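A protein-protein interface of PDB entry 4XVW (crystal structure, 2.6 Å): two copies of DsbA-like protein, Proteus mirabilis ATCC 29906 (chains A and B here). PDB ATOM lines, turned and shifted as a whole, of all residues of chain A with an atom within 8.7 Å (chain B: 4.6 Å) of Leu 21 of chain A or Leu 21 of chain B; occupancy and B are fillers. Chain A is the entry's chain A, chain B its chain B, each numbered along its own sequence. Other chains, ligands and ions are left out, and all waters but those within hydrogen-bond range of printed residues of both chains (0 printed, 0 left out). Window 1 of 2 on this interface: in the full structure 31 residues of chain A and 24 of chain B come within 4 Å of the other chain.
OG of Ser 23 of chain A sits at hydrogen-bond distance from O of Thr 20 of chain A (3.5 Å).
CG2 of Val 17 of chain B touches CG2 of Val 17 of chain A (3.8 Å).
Val 17 of chain B touches Thr 20 of chain A.
Leu 21 of chain A touches Leu 21 of chain B.
Arg 18 of chain B touches Asn 24 of chain A.
NH1 of Arg 18 of chain B touches CG1 of Ile 27 of chain A (3.2 Å).
Glu 30 of chain A touches Val 22 of chain B.
Pro 25 of chain B touches Ala 34 of chain A (CG to O, 3.8 Å).
Leu 35 of chain A touches Pro 25 of chain B (CD1 to O, 3.0 Å).
OD1 of Asn 24 of chain B touches NZ of Lys 38 of chain A, at 3.9 Å.
Lys 38 of chain A touches Pro 25 of chain B (CD to CD, 3.6 Å).
Of chain B, only Leu 21 comes within 4 Å of Leu 21 of chain A.
Of chain A, only Leu 21 comes within 4 Å of Leu 21 of chain B.
No residue of chain A comes within 4 Å of Thr 20 of chain B.
Of the printed residues of chain B, Ile 27 of chain A touches Arg 18.
Of the printed residues of chain A, Asn 24 of chain B touches Lys 38 (3.9 Å).
Printed residues of chain B within 4 Å of Val 17 of chain A: Val 17 (3.8 Å).
The nearest residue of chain A that does not touch Leu 21 of chain B is Ala 31 of chain A (4.1 Å).
Of the 11 printed residues of chain B, 6 touch a printed residue of chain A.
Hydrophobic or aromatic side chains of chain B within 4 Å of the printed part of chain A: Val 17, Leu 21, Val 22 and Pro 25.
Of the 22 printed residues of chain A, 9 touch a printed residue of chain B.
Hydrophobic or aromatic side chains of chain A that line the printed part of chain B: Val 17, Leu 21, Ile 27 and Leu 35.
Among the printed residues, no Asp or Glu carboxylate lies within 4 Å of a Lys or Arg side-chain nitrogen of the other chain.
Val 17 of chain B touches its own counterpart, Val 17 of chain A.
Thr 20 of chain A touches Val 17 of chain B, but with the chains exchanged Val 17 of chain A does not touch Thr 20 of chain B (9.1 Å).
Leu 21 of chain A touches its own counterpart, Leu 21 of chain B.
Ile 27 of chain A touches Arg 18 of chain B, but with the chains exchanged Arg 18 of chain A does not touch Ile 27 of chain B (12.0 Å).
Positions printed for both chains: 16, 17, 18, 19, 20, 21, 22, 23, 24, 25 and 27.
Of the 10 pairs that touch across the chains among the printed residues, 2 have their exchanged pair printed and touching as well.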
ATOM      1  N   ARG A  14       0.293 -10.908  -1.704  1.00  0.00           N
ATOM      2  CA  ARG A  14       0.183 -10.738  -3.146  1.00  0.00           C
ATOM      3  C   ARG A  14      -0.911 -11.625  -3.735  1.00  0.00           C
ATOM      4  O   ARG A  14      -1.496 -11.299  -4.768  1.00  0.00           O
ATOM      5  CB  ARG A  14       1.517 -11.048  -3.827  1.00  0.00           C
ATOM      6  CG  ARG A  14       2.634 -10.072  -3.509  1.00  0.00           C
ATOM      7  CD  ARG A  14       3.898 -10.445  -4.268  1.00  0.00           C
ATOM      8  NE  ARG A  14       5.004  -9.525  -4.006  1.00  0.00           N
ATOM      9  CZ  ARG A  14       5.242  -8.415  -4.699  1.00  0.00           C
ATOM     10  NH1 ARG A  14       4.456  -8.068  -5.713  1.00  0.00           N
ATOM     11  NH2 ARG A  14       6.275  -7.647  -4.382  1.00  0.00           N
ATOM     12  N   ALA A  15      -1.178 -12.748  -3.079  1.00  0.00           N
ATOM     13  CA  ALA A  15      -2.232 -13.654  -3.520  1.00  0.00           C
ATOM     14  C   ALA A  15      -3.616 -13.191  -3.084  1.00  0.00           C
ATOM     15  O   ALA A  15      -4.596 -13.374  -3.808  1.00  0.00           O
ATOM     16  CB  ALA A  15      -1.963 -15.055  -2.995  1.00  0.00           C
ATOM     17  N   LEU A  16      -3.696 -12.586  -1.904  1.00  0.00           N
ATOM     18  CA  LEU A  16      -4.977 -12.148  -1.364  1.00  0.00           C
ATOM     19  C   LEU A  16      -5.567 -10.969  -2.124  1.00  0.00           C
ATOM     20  O   LEU A  16      -6.779 -10.894  -2.303  1.00  0.00           O
ATOM     21  CB  LEU A  16      -4.823 -11.780   0.113  1.00  0.00           C
ATOM     22  CG  LEU A  16      -4.645 -12.946   1.089  1.00  0.00           C
ATOM     23  CD1 LEU A  16      -4.276 -12.434   2.473  1.00  0.00           C
ATOM     24  CD2 LEU A  16      -5.906 -13.791   1.156  1.00  0.00           C
ATOM     25  N   VAL A  17      -4.713 -10.063  -2.585  1.00  0.00           N
ATOM     26  CA  VAL A  17      -5.170  -8.919  -3.368  1.00  0.00           C
ATOM     27  C   VAL A  17      -5.874  -9.384  -4.639  1.00  0.00           C
ATOM     28  O   VAL A  17      -6.868  -8.788  -5.053  1.00  0.00           O
ATOM     29  CB  VAL A  17      -4.010  -7.952  -3.728  1.00  0.00           C
ATOM     30  CG1 VAL A  17      -2.815  -8.705  -4.283  1.00  0.00           C
ATOM     31  CG2 VAL A  17      -4.475  -6.882  -4.718  1.00  0.00           C
ATOM     32  N   ARG A  18      -5.365 -10.446  -5.257  1.00  0.00           N
ATOM     33  CA  ARG A  18      -5.996 -10.975  -6.460  1.00  0.00           C
ATOM     34  C   ARG A  18      -7.350 -11.546  -6.067  1.00  0.00           C
ATOM     35  O   ARG A  18      -8.371 -11.233  -6.672  1.00  0.00           O
ATOM     36  CB  ARG A  18      -5.149 -12.075  -7.104  1.00  0.00           C
ATOM     37  CG  ARG A  18      -5.648 -12.523  -8.477  1.00  0.00           C
ATOM     38  CD  ARG A  18      -4.937 -13.774  -8.967  1.00  0.00           C
ATOM     39  NE  ARG A  18      -5.610 -14.986  -8.494  1.00  0.00           N
ATOM     40  CZ  ARG A  18      -6.605 -15.585  -9.149  1.00  0.00           C
ATOM     41  NH1 ARG A  18      -7.027 -15.103 -10.311  1.00  0.00           N
ATOM     42  NH2 ARG A  18      -7.175 -16.677  -8.657  1.00  0.00           N
ATOM     43  N   ASP A  19      -7.344 -12.370  -5.025  1.00  0.00           N
ATOM     44  CA  ASP A  19      -8.546 -13.054  -4.571  1.00  0.00           C
ATOM     45  C   ASP A  19      -9.602 -12.060  -4.116  1.00  0.00           C
ATOM     46  O   ASP A  19     -10.791 -12.242  -4.370  1.00  0.00           O
ATOM     47  CB  ASP A  19      -8.216 -14.022  -3.435  1.00  0.00           C
ATOM     48  CG  ASP A  19      -9.421 -14.830  -2.986  1.00  0.00           C
ATOM     49  OD1 ASP A  19     -10.402 -14.924  -3.752  1.00  0.00           O
ATOM     50  OD2 ASP A  19      -9.385 -15.375  -1.864  1.00  0.00           O
ATOM     51  N   THR A  20      -9.161 -11.006  -3.441  1.00  0.00           N
ATOM     52  CA  THR A  20     -10.082 -10.038  -2.869  1.00  0.00           C
ATOM     53  C   THR A  20     -10.798  -9.289  -3.977  1.00  0.00           C
ATOM     54  O   THR A  20     -12.001  -9.037  -3.902  1.00  0.00           O
ATOM     55  CB  THR A  20      -9.351  -9.015  -1.983  1.00  0.00           C
ATOM     56  OG1 THR A  20      -8.456  -9.690  -1.095  1.00  0.00           O
ATOM     57  CG2 THR A  20     -10.347  -8.181  -1.189  1.00  0.00           C
ATOM     58  N   LEU A  21     -10.040  -8.943  -5.010  1.00  0.00           N
ATOM     59  CA  LEU A  21     -10.563  -8.158  -6.113  1.00  0.00           C
ATOM     60  C   LEU A  21     -11.465  -9.006  -7.000  1.00  0.00           C
ATOM     61  O   LEU A  21     -12.426  -8.505  -7.577  1.00  0.00           O
ATOM     62  CB  LEU A  21      -9.412  -7.563  -6.927  1.00  0.00           C
ATOM     63  CG  LEU A  21      -8.717  -6.339  -6.318  1.00  0.00           C
ATOM     64  CD1 LEU A  21      -7.568  -5.897  -7.202  1.00  0.00           C
ATOM     65  CD2 LEU A  21      -9.682  -5.180  -6.092  1.00  0.00           C
ATOM     66  N   VAL A  22     -11.150 -10.291  -7.110  1.00  0.00           N
ATOM     67  CA  VAL A  22     -11.924 -11.196  -7.953  1.00  0.00           C
ATOM     68  C   VAL A  22     -13.131 -11.769  -7.205  1.00  0.00           C
ATOM     69  O   VAL A  22     -14.206 -11.921  -7.785  1.00  0.00           O
ATOM     70  CB  VAL A  22     -11.041 -12.341  -8.494  1.00  0.00           C
ATOM     71  CG1 VAL A  22     -11.865 -13.330  -9.305  1.00  0.00           C
ATOM     72  CG2 VAL A  22      -9.907 -11.778  -9.346  1.00  0.00           C
ATOM     73  N   SER A  23     -12.957 -12.094  -5.927  1.00  0.00           N
ATOM     74  CA  SER A  23     -14.065 -12.607  -5.124  1.00  0.00           C
ATOM     75  C   SER A  23     -15.097 -11.513  -4.841  1.00  0.00           C
ATOM     76  O   SER A  23     -16.298 -11.778  -4.833  1.00  0.00           O
ATOM     77  CB  SER A  23     -13.553 -13.196  -3.811  1.00  0.00           C
ATOM     78  OG  SER A  23     -13.088 -12.180  -2.941  1.00  0.00           O
ATOM     79  N   ASN A  24     -14.618 -10.294  -4.598  1.00  0.00           N
ATOM     80  CA  ASN A  24     -15.482  -9.129  -4.398  1.00  0.00           C
ATOM     81  C   ASN A  24     -15.141  -8.029  -5.404  1.00  0.00           C
ATOM     82  O   ASN A  24     -14.427  -7.082  -5.076  1.00  0.00           O
ATOM     83  CB  ASN A  24     -15.358  -8.602  -2.966  1.00  0.00           C
ATOM     84  CG  ASN A  24     -16.542  -7.747  -2.558  1.00  0.00           C
ATOM     85  OD1 ASN A  24     -16.709  -6.628  -3.041  1.00  0.00           O
ATOM     86  ND2 ASN A  24     -17.376  -8.274  -1.673  1.00  0.00           N
ATOM     87  N   PRO A  25     -15.656  -8.152  -6.639  1.00  0.00           N
ATOM     88  CA  PRO A  25     -15.324  -7.201  -7.709  1.00  0.00           C
ATOM     89  C   PRO A  25     -15.902  -5.801  -7.519  1.00  0.00           C
ATOM     90  O   PRO A  25     -15.434  -4.859  -8.158  1.00  0.00           O
ATOM     91  CB  PRO A  25     -15.947  -7.851  -8.955  1.00  0.00           C
ATOM     92  CG  PRO A  25     -16.218  -9.275  -8.576  1.00  0.00           C
ATOM     93  CD  PRO A  25     -16.528  -9.233  -7.124  1.00  0.00           C
ATOM     94  N   GLU A  26     -16.880  -5.663  -6.632  1.00  0.00           N
ATOM     95  CA  GLU A  26     -17.520  -4.373  -6.395  1.00  0.00           C
ATOM     96  C   GLU A  26     -16.555  -3.397  -5.735  1.00  0.00           C
ATOM     97  O   GLU A  26     -16.745  -2.182  -5.800  1.00  0.00           O
ATOM     98  CB  GLU A  26     -18.786  -4.548  -5.560  1.00  0.00           C
ATOM     99  CG  GLU A  26     -19.820  -5.427  -6.251  1.00  0.00           C
ATOM    100  CD  GLU A  26     -21.035  -5.701  -5.392  1.00  0.00           C
ATOM    101  OE1 GLU A  26     -20.943  -5.530  -4.159  1.00  0.00           O
ATOM    102  OE2 GLU A  26     -22.082  -6.087  -5.956  1.00  0.00           O
ATOM    103  N   ILE A  27     -15.520  -3.939  -5.104  1.00  0.00           N
ATOM    104  CA  ILE A  27     -14.458  -3.124  -4.534  1.00  0.00           C
ATOM    105  C   ILE A  27     -13.868  -2.253  -5.626  1.00  0.00           C
ATOM    106  O   ILE A  27     -13.477  -1.112  -5.383  1.00  0.00           O
ATOM    107  CB  ILE A  27     -13.342  -3.987  -3.913  1.00  0.00           C
ATOM    108  CG1 ILE A  27     -13.901  -4.812  -2.753  1.00  0.00           C
ATOM    109  CG2 ILE A  27     -12.173  -3.108  -3.453  1.00  0.00           C
ATOM    110  CD1 ILE A  27     -12.895  -5.744  -2.106  1.00  0.00           C
ATOM    111  N   LEU A  28     -13.809  -2.799  -6.834  1.00  0.00           N
ATOM    112  CA  LEU A  28     -13.200  -2.094  -7.946  1.00  0.00           C
ATOM    113  C   LEU A  28     -14.013  -0.876  -8.371  1.00  0.00           C
ATOM    114  O   LEU A  28     -13.488   0.235  -8.381  1.00  0.00           O
ATOM    115  CB  LEU A  28     -13.036  -3.045  -9.130  1.00  0.00           C
ATOM    116  CG  LEU A  28     -12.259  -2.520 -10.336  1.00  0.00           C
ATOM    117  CD1 LEU A  28     -10.817  -2.213  -9.973  1.00  0.00           C
ATOM    118  CD2 LEU A  28     -12.327  -3.533 -11.468  1.00  0.00           C
ATOM    119  N   GLU A  29     -15.294  -1.069  -8.676  1.00  0.00           N
ATOM    120  CA  GLU A  29     -16.125   0.035  -9.154  1.00  0.00           C
ATOM    121  C   GLU A  29     -16.236   1.116  -8.089  1.00  0.00           C
ATOM    122  O   GLU A  29     -16.456   2.287  -8.400  1.00  0.00           O
ATOM    123  CB  GLU A  29     -17.521  -0.435  -9.578  1.00  0.00           C
ATOM    124  CG  GLU A  29     -18.380  -1.050  -8.488  1.00  0.00           C
ATOM    125  CD  GLU A  29     -19.817  -1.268  -8.940  1.00  0.00           C
ATOM    126  OE1 GLU A  29     -20.222  -0.680  -9.966  1.00  0.00           O
ATOM    127  OE2 GLU A  29     -20.548  -2.024  -8.265  1.00  0.00           O
ATOM    128  N   GLU A  30     -16.072   0.721  -6.832  1.00  0.00           N
ATOM    129  CA  GLU A  30     -16.095   1.673  -5.736  1.00  0.00           C
ATOM    130  C   GLU A  30     -14.897   2.597  -5.862  1.00  0.00           C
ATOM    131  O   GLU A  30     -15.001   3.803  -5.642  1.00  0.00           O
ATOM    132  CB  GLU A  30     -16.053   0.945  -4.393  1.00  0.00           C
ATOM    133  CG  GLU A  30     -16.112   1.858  -3.176  1.00  0.00           C
ATOM    134  CD  GLU A  30     -16.089   1.090  -1.866  1.00  0.00           C
ATOM    135  OE1 GLU A  30     -16.262  -0.147  -1.892  1.00  0.00           O
ATOM    136  OE2 GLU A  30     -15.897   1.727  -0.808  1.00  0.00           O
ATOM    137  N   ALA A  31     -13.760   2.017  -6.227  1.00  0.00           N
ATOM    138  CA  ALA A  31     -12.532   2.775  -6.399  1.00  0.00           C
ATOM    139  C   ALA A  31     -12.556   3.544  -7.715  1.00  0.00           C
ATOM    140  O   ALA A  31     -11.862   4.547  -7.865  1.00  0.00           O
ATOM    141  CB  ALA A  31     -11.329   1.855  -6.340  1.00  0.00           C
ATOM    142  N   ILE A  32     -13.362   3.075  -8.665  1.00  0.00           N
ATOM    143  CA  ILE A  32     -13.485   3.750  -9.952  1.00  0.00           C
ATOM    144  C   ILE A  32     -14.183   5.096  -9.794  1.00  0.00           C
ATOM    145  O   ILE A  32     -13.690   6.108 -10.288  1.00  0.00           O
ATOM    146  CB  ILE A  32     -14.249   2.887 -10.990  1.00  0.00           C
ATOM    147  CG1 ILE A  32     -13.448   1.622 -11.315  1.00  0.00           C
ATOM    148  CG2 ILE A  32     -14.467   3.665 -12.285  1.00  0.00           C
ATOM    149  CD1 ILE A  32     -14.149   0.628 -12.242  1.00  0.00           C
ATOM    150  N   ALA A  34     -14.630   6.586  -6.930  1.00  0.00           N
ATOM    151  CA  ALA A  34     -13.905   7.311  -5.896  1.00  0.00           C
ATOM    152  C   ALA A  34     -12.798   8.132  -6.523  1.00  0.00           C
ATOM    153  O   ALA A  34     -12.442   9.204  -6.036  1.00  0.00           O
ATOM    154  CB  ALA A  34     -13.322   6.345  -4.875  1.00  0.00           C
ATOM    155  N   LEU A  35     -12.255   7.612  -7.615  1.00  0.00           N
ATOM    156  CA  LEU A  35     -11.208   8.300  -8.341  1.00  0.00           C
ATOM    157  C   LEU A  35     -11.808   9.389  -9.228  1.00  0.00           C
ATOM    158  O   LEU A  35     -11.273  10.495  -9.307  1.00  0.00           O
ATOM    159  CB  LEU A  35     -10.379   7.303  -9.139  1.00  0.00           C
ATOM    160  CG  LEU A  35      -9.225   7.970  -9.874  1.00  0.00           C
ATOM    161  CD1 LEU A  35      -8.024   7.084  -9.832  1.00  0.00           C
ATOM    162  CD2 LEU A  35      -9.564   8.261 -11.291  1.00  0.00           C
ATOM    163  N   LYS A  38     -12.212  11.953  -6.982  1.00  0.00           N
ATOM    164  CA  LYS A  38     -10.940  12.566  -6.634  1.00  0.00           C
ATOM    165  C   LYS A  38     -10.389  13.394  -7.792  1.00  0.00           C
ATOM    166  O   LYS A  38      -9.745  14.417  -7.566  1.00  0.00           O
ATOM    167  CB  LYS A  38      -9.936  11.498  -6.200  1.00  0.00           C
ATOM    168  CG  LYS A  38      -8.599  12.056  -5.746  1.00  0.00           C
ATOM    169  CD  LYS A  38      -7.725  10.960  -5.157  1.00  0.00           C
ATOM    170  CE  LYS A  38      -6.403  11.506  -4.634  1.00  0.00           C
ATOM    171  NZ  LYS A  38      -5.584  10.458  -3.954  1.00  0.00           N
ATOM    172  N   LEU B  16      -7.702  -4.195   4.173  1.00  0.00           N
ATOM    173  CA  LEU B  16      -6.710  -3.184   3.848  1.00  0.00           C
ATOM    174  C   LEU B  16      -6.570  -2.942   2.349  1.00  0.00           C
ATOM    175  O   LEU B  16      -6.428  -1.801   1.915  1.00  0.00           O
ATOM    176  CB  LEU B  16      -5.354  -3.594   4.417  1.00  0.00           C
ATOM    177  CG  LEU B  16      -5.182  -3.504   5.934  1.00  0.00           C
ATOM    178  CD1 LEU B  16      -3.867  -4.152   6.341  1.00  0.00           C
ATOM    179  CD2 LEU B  16      -5.253  -2.065   6.415  1.00  0.00           C
ATOM    180  N   VAL B  17      -6.622  -4.009   1.558  1.00  0.00           N
ATOM    181  CA  VAL B  17      -6.558  -3.871   0.106  1.00  0.00           C
ATOM    182  C   VAL B  17      -7.763  -3.077  -0.362  1.00  0.00           C
ATOM    183  O   VAL B  17      -7.663  -2.234  -1.254  1.00  0.00           O
ATOM    184  CB  VAL B  17      -6.499  -5.240  -0.625  1.00  0.00           C
ATOM    185  CG1 VAL B  17      -7.604  -6.171  -0.152  1.00  0.00           C
ATOM    186  CG2 VAL B  17      -6.608  -5.049  -2.135  1.00  0.00           C
ATOM    187  N   ARG B  18      -8.901  -3.354   0.258  1.00  0.00           N
ATOM    188  CA  ARG B  18     -10.134  -2.660  -0.061  1.00  0.00           C
ATOM    189  C   ARG B  18     -10.004  -1.213   0.388  1.00  0.00           C
ATOM    190  O   ARG B  18     -10.255  -0.283  -0.374  1.00  0.00           O
ATOM    191  CB  ARG B  18     -11.313  -3.322   0.653  1.00  0.00           C
ATOM    192  CG  ARG B  18     -12.686  -2.821   0.248  1.00  0.00           C
ATOM    193  CD  ARG B  18     -13.753  -3.367   1.192  1.00  0.00           C
ATOM    194  NE  ARG B  18     -15.115  -3.183   0.690  1.00  0.00           N
ATOM    195  CZ  ARG B  18     -15.858  -4.147   0.144  1.00  0.00           C
ATOM    196  NH1 ARG B  18     -15.400  -5.392   0.047  1.00  0.00           N
ATOM    197  NH2 ARG B  18     -17.081  -3.873  -0.286  1.00  0.00           N
ATOM    198  N   ASP B  19      -9.584  -1.043   1.636  1.00  0.00           N
ATOM    199  CA  ASP B  19      -9.479   0.273   2.256  1.00  0.00           C
ATOM    200  C   ASP B  19      -8.438   1.164   1.577  1.00  0.00           C
ATOM    201  O   ASP B  19      -8.669   2.355   1.368  1.00  0.00           O
ATOM    202  CB  ASP B  19      -9.142   0.116   3.741  1.00  0.00           C
ATOM    203  CG  ASP B  19      -9.125   1.437   4.484  1.00  0.00           C
ATOM    204  OD1 ASP B  19      -9.716   2.417   3.982  1.00  0.00           O
ATOM    205  OD2 ASP B  19      -8.520   1.494   5.575  1.00  0.00           O
ATOM    206  N   THR B  20      -7.297   0.580   1.228  1.00  0.00           N
ATOM    207  CA  THR B  20      -6.182   1.341   0.665  1.00  0.00           C
ATOM    208  C   THR B  20      -6.495   1.873  -0.729  1.00  0.00           C
ATOM    209  O   THR B  20      -6.127   2.997  -1.070  1.00  0.00           O
ATOM    210  CB  THR B  20      -4.900   0.493   0.599  1.00  0.00           C
ATOM    211  OG1 THR B  20      -4.651  -0.104   1.877  1.00  0.00           O
ATOM    212  CG2 THR B  20      -3.706   1.356   0.219  1.00  0.00           C
ATOM    213  N   LEU B  21      -7.182   1.066  -1.529  1.00  0.00           N
ATOM    214  CA  LEU B  21      -7.463   1.425  -2.912  1.00  0.00           C
ATOM    215  C   LEU B  21      -8.474   2.561  -2.971  1.00  0.00           C
ATOM    216  O   LEU B  21      -8.463   3.358  -3.903  1.00  0.00           O
ATOM    217  CB  LEU B  21      -7.990   0.218  -3.693  1.00  0.00           C
ATOM    218  CG  LEU B  21      -6.982  -0.833  -4.165  1.00  0.00           C
ATOM    219  CD1 LEU B  21      -7.711  -1.960  -4.881  1.00  0.00           C
ATOM    220  CD2 LEU B  21      -5.916  -0.231  -5.069  1.00  0.00           C
ATOM    221  N   VAL B  22      -9.353   2.625  -1.977  1.00  0.00           N
ATOM    222  CA  VAL B  22     -10.404   3.637  -1.947  1.00  0.00           C
ATOM    223  C   VAL B  22      -9.912   4.962  -1.352  1.00  0.00           C
ATOM    224  O   VAL B  22     -10.279   6.033  -1.834  1.00  0.00           O
ATOM    225  CB  VAL B  22     -11.620   3.125  -1.151  1.00  0.00           C
ATOM    226  CG1 VAL B  22     -12.707   4.190  -1.065  1.00  0.00           C
ATOM    227  CG2 VAL B  22     -12.170   1.862  -1.798  1.00  0.00           C
ATOM    228  N   SER B  23      -9.085   4.893  -0.313  1.00  0.00           N
ATOM    229  CA  SER B  23      -8.524   6.099   0.294  1.00  0.00           C
ATOM    230  C   SER B  23      -7.538   6.752  -0.669  1.00  0.00           C
ATOM    231  O   SER B  23      -7.428   7.978  -0.731  1.00  0.00           O
ATOM    232  CB  SER B  23      -7.840   5.778   1.623  1.00  0.00           C
ATOM    233  OG  SER B  23      -6.642   5.052   1.416  1.00  0.00           O
ATOM    234  N   ASN B  24      -6.818   5.912  -1.406  1.00  0.00           N
ATOM    235  CA  ASN B  24      -5.890   6.353  -2.443  1.00  0.00           C
ATOM    236  C   ASN B  24      -6.314   5.771  -3.786  1.00  0.00           C
ATOM    237  O   ASN B  24      -5.770   4.760  -4.228  1.00  0.00           O
ATOM    238  CB  ASN B  24      -4.454   5.926  -2.122  1.00  0.00           C
ATOM    239  CG  ASN B  24      -3.420   6.734  -2.884  1.00  0.00           C
ATOM    240  OD1 ASN B  24      -3.621   7.076  -4.048  1.00  0.00           O
ATOM    241  ND2 ASN B  24      -2.286   6.999  -2.247  1.00  0.00           N
ATOM    242  N   PRO B  25      -7.295   6.405  -4.444  1.00  0.00           N
ATOM    243  CA  PRO B  25      -7.766   5.844  -5.713  1.00  0.00           C
ATOM    244  C   PRO B  25      -6.721   5.937  -6.815  1.00  0.00           C
ATOM    245  O   PRO B  25      -6.810   5.215  -7.806  1.00  0.00           O
ATOM    246  CB  PRO B  25      -8.981   6.720  -6.055  1.00  0.00           C
ATOM    247  CG  PRO B  25      -9.353   7.408  -4.780  1.00  0.00           C
ATOM    248  CD  PRO B  25      -8.066   7.595  -4.052  1.00  0.00           C
ATOM    249  N   ILE B  27      -3.808   4.830  -6.894  1.00  0.00           N
ATOM    250  CA  ILE B  27      -3.137   3.549  -7.081  1.00  0.00           C
ATOM    251  C   ILE B  27      -3.737   2.828  -8.271  1.00  0.00           C
ATOM    252  O   ILE B  27      -3.036   2.172  -9.042  1.00  0.00           O
ATOM    253  CB  ILE B  27      -3.262   2.642  -5.836  1.00  0.00           C
ATOM    254  CG1 ILE B  27      -2.565   3.291  -4.637  1.00  0.00           C
ATOM    255  CG2 ILE B  27      -2.703   1.239  -6.128  1.00  0.00           C
ATOM    256  CD1 ILE B  27      -2.674   2.498  -3.347  1.00  0.00           C
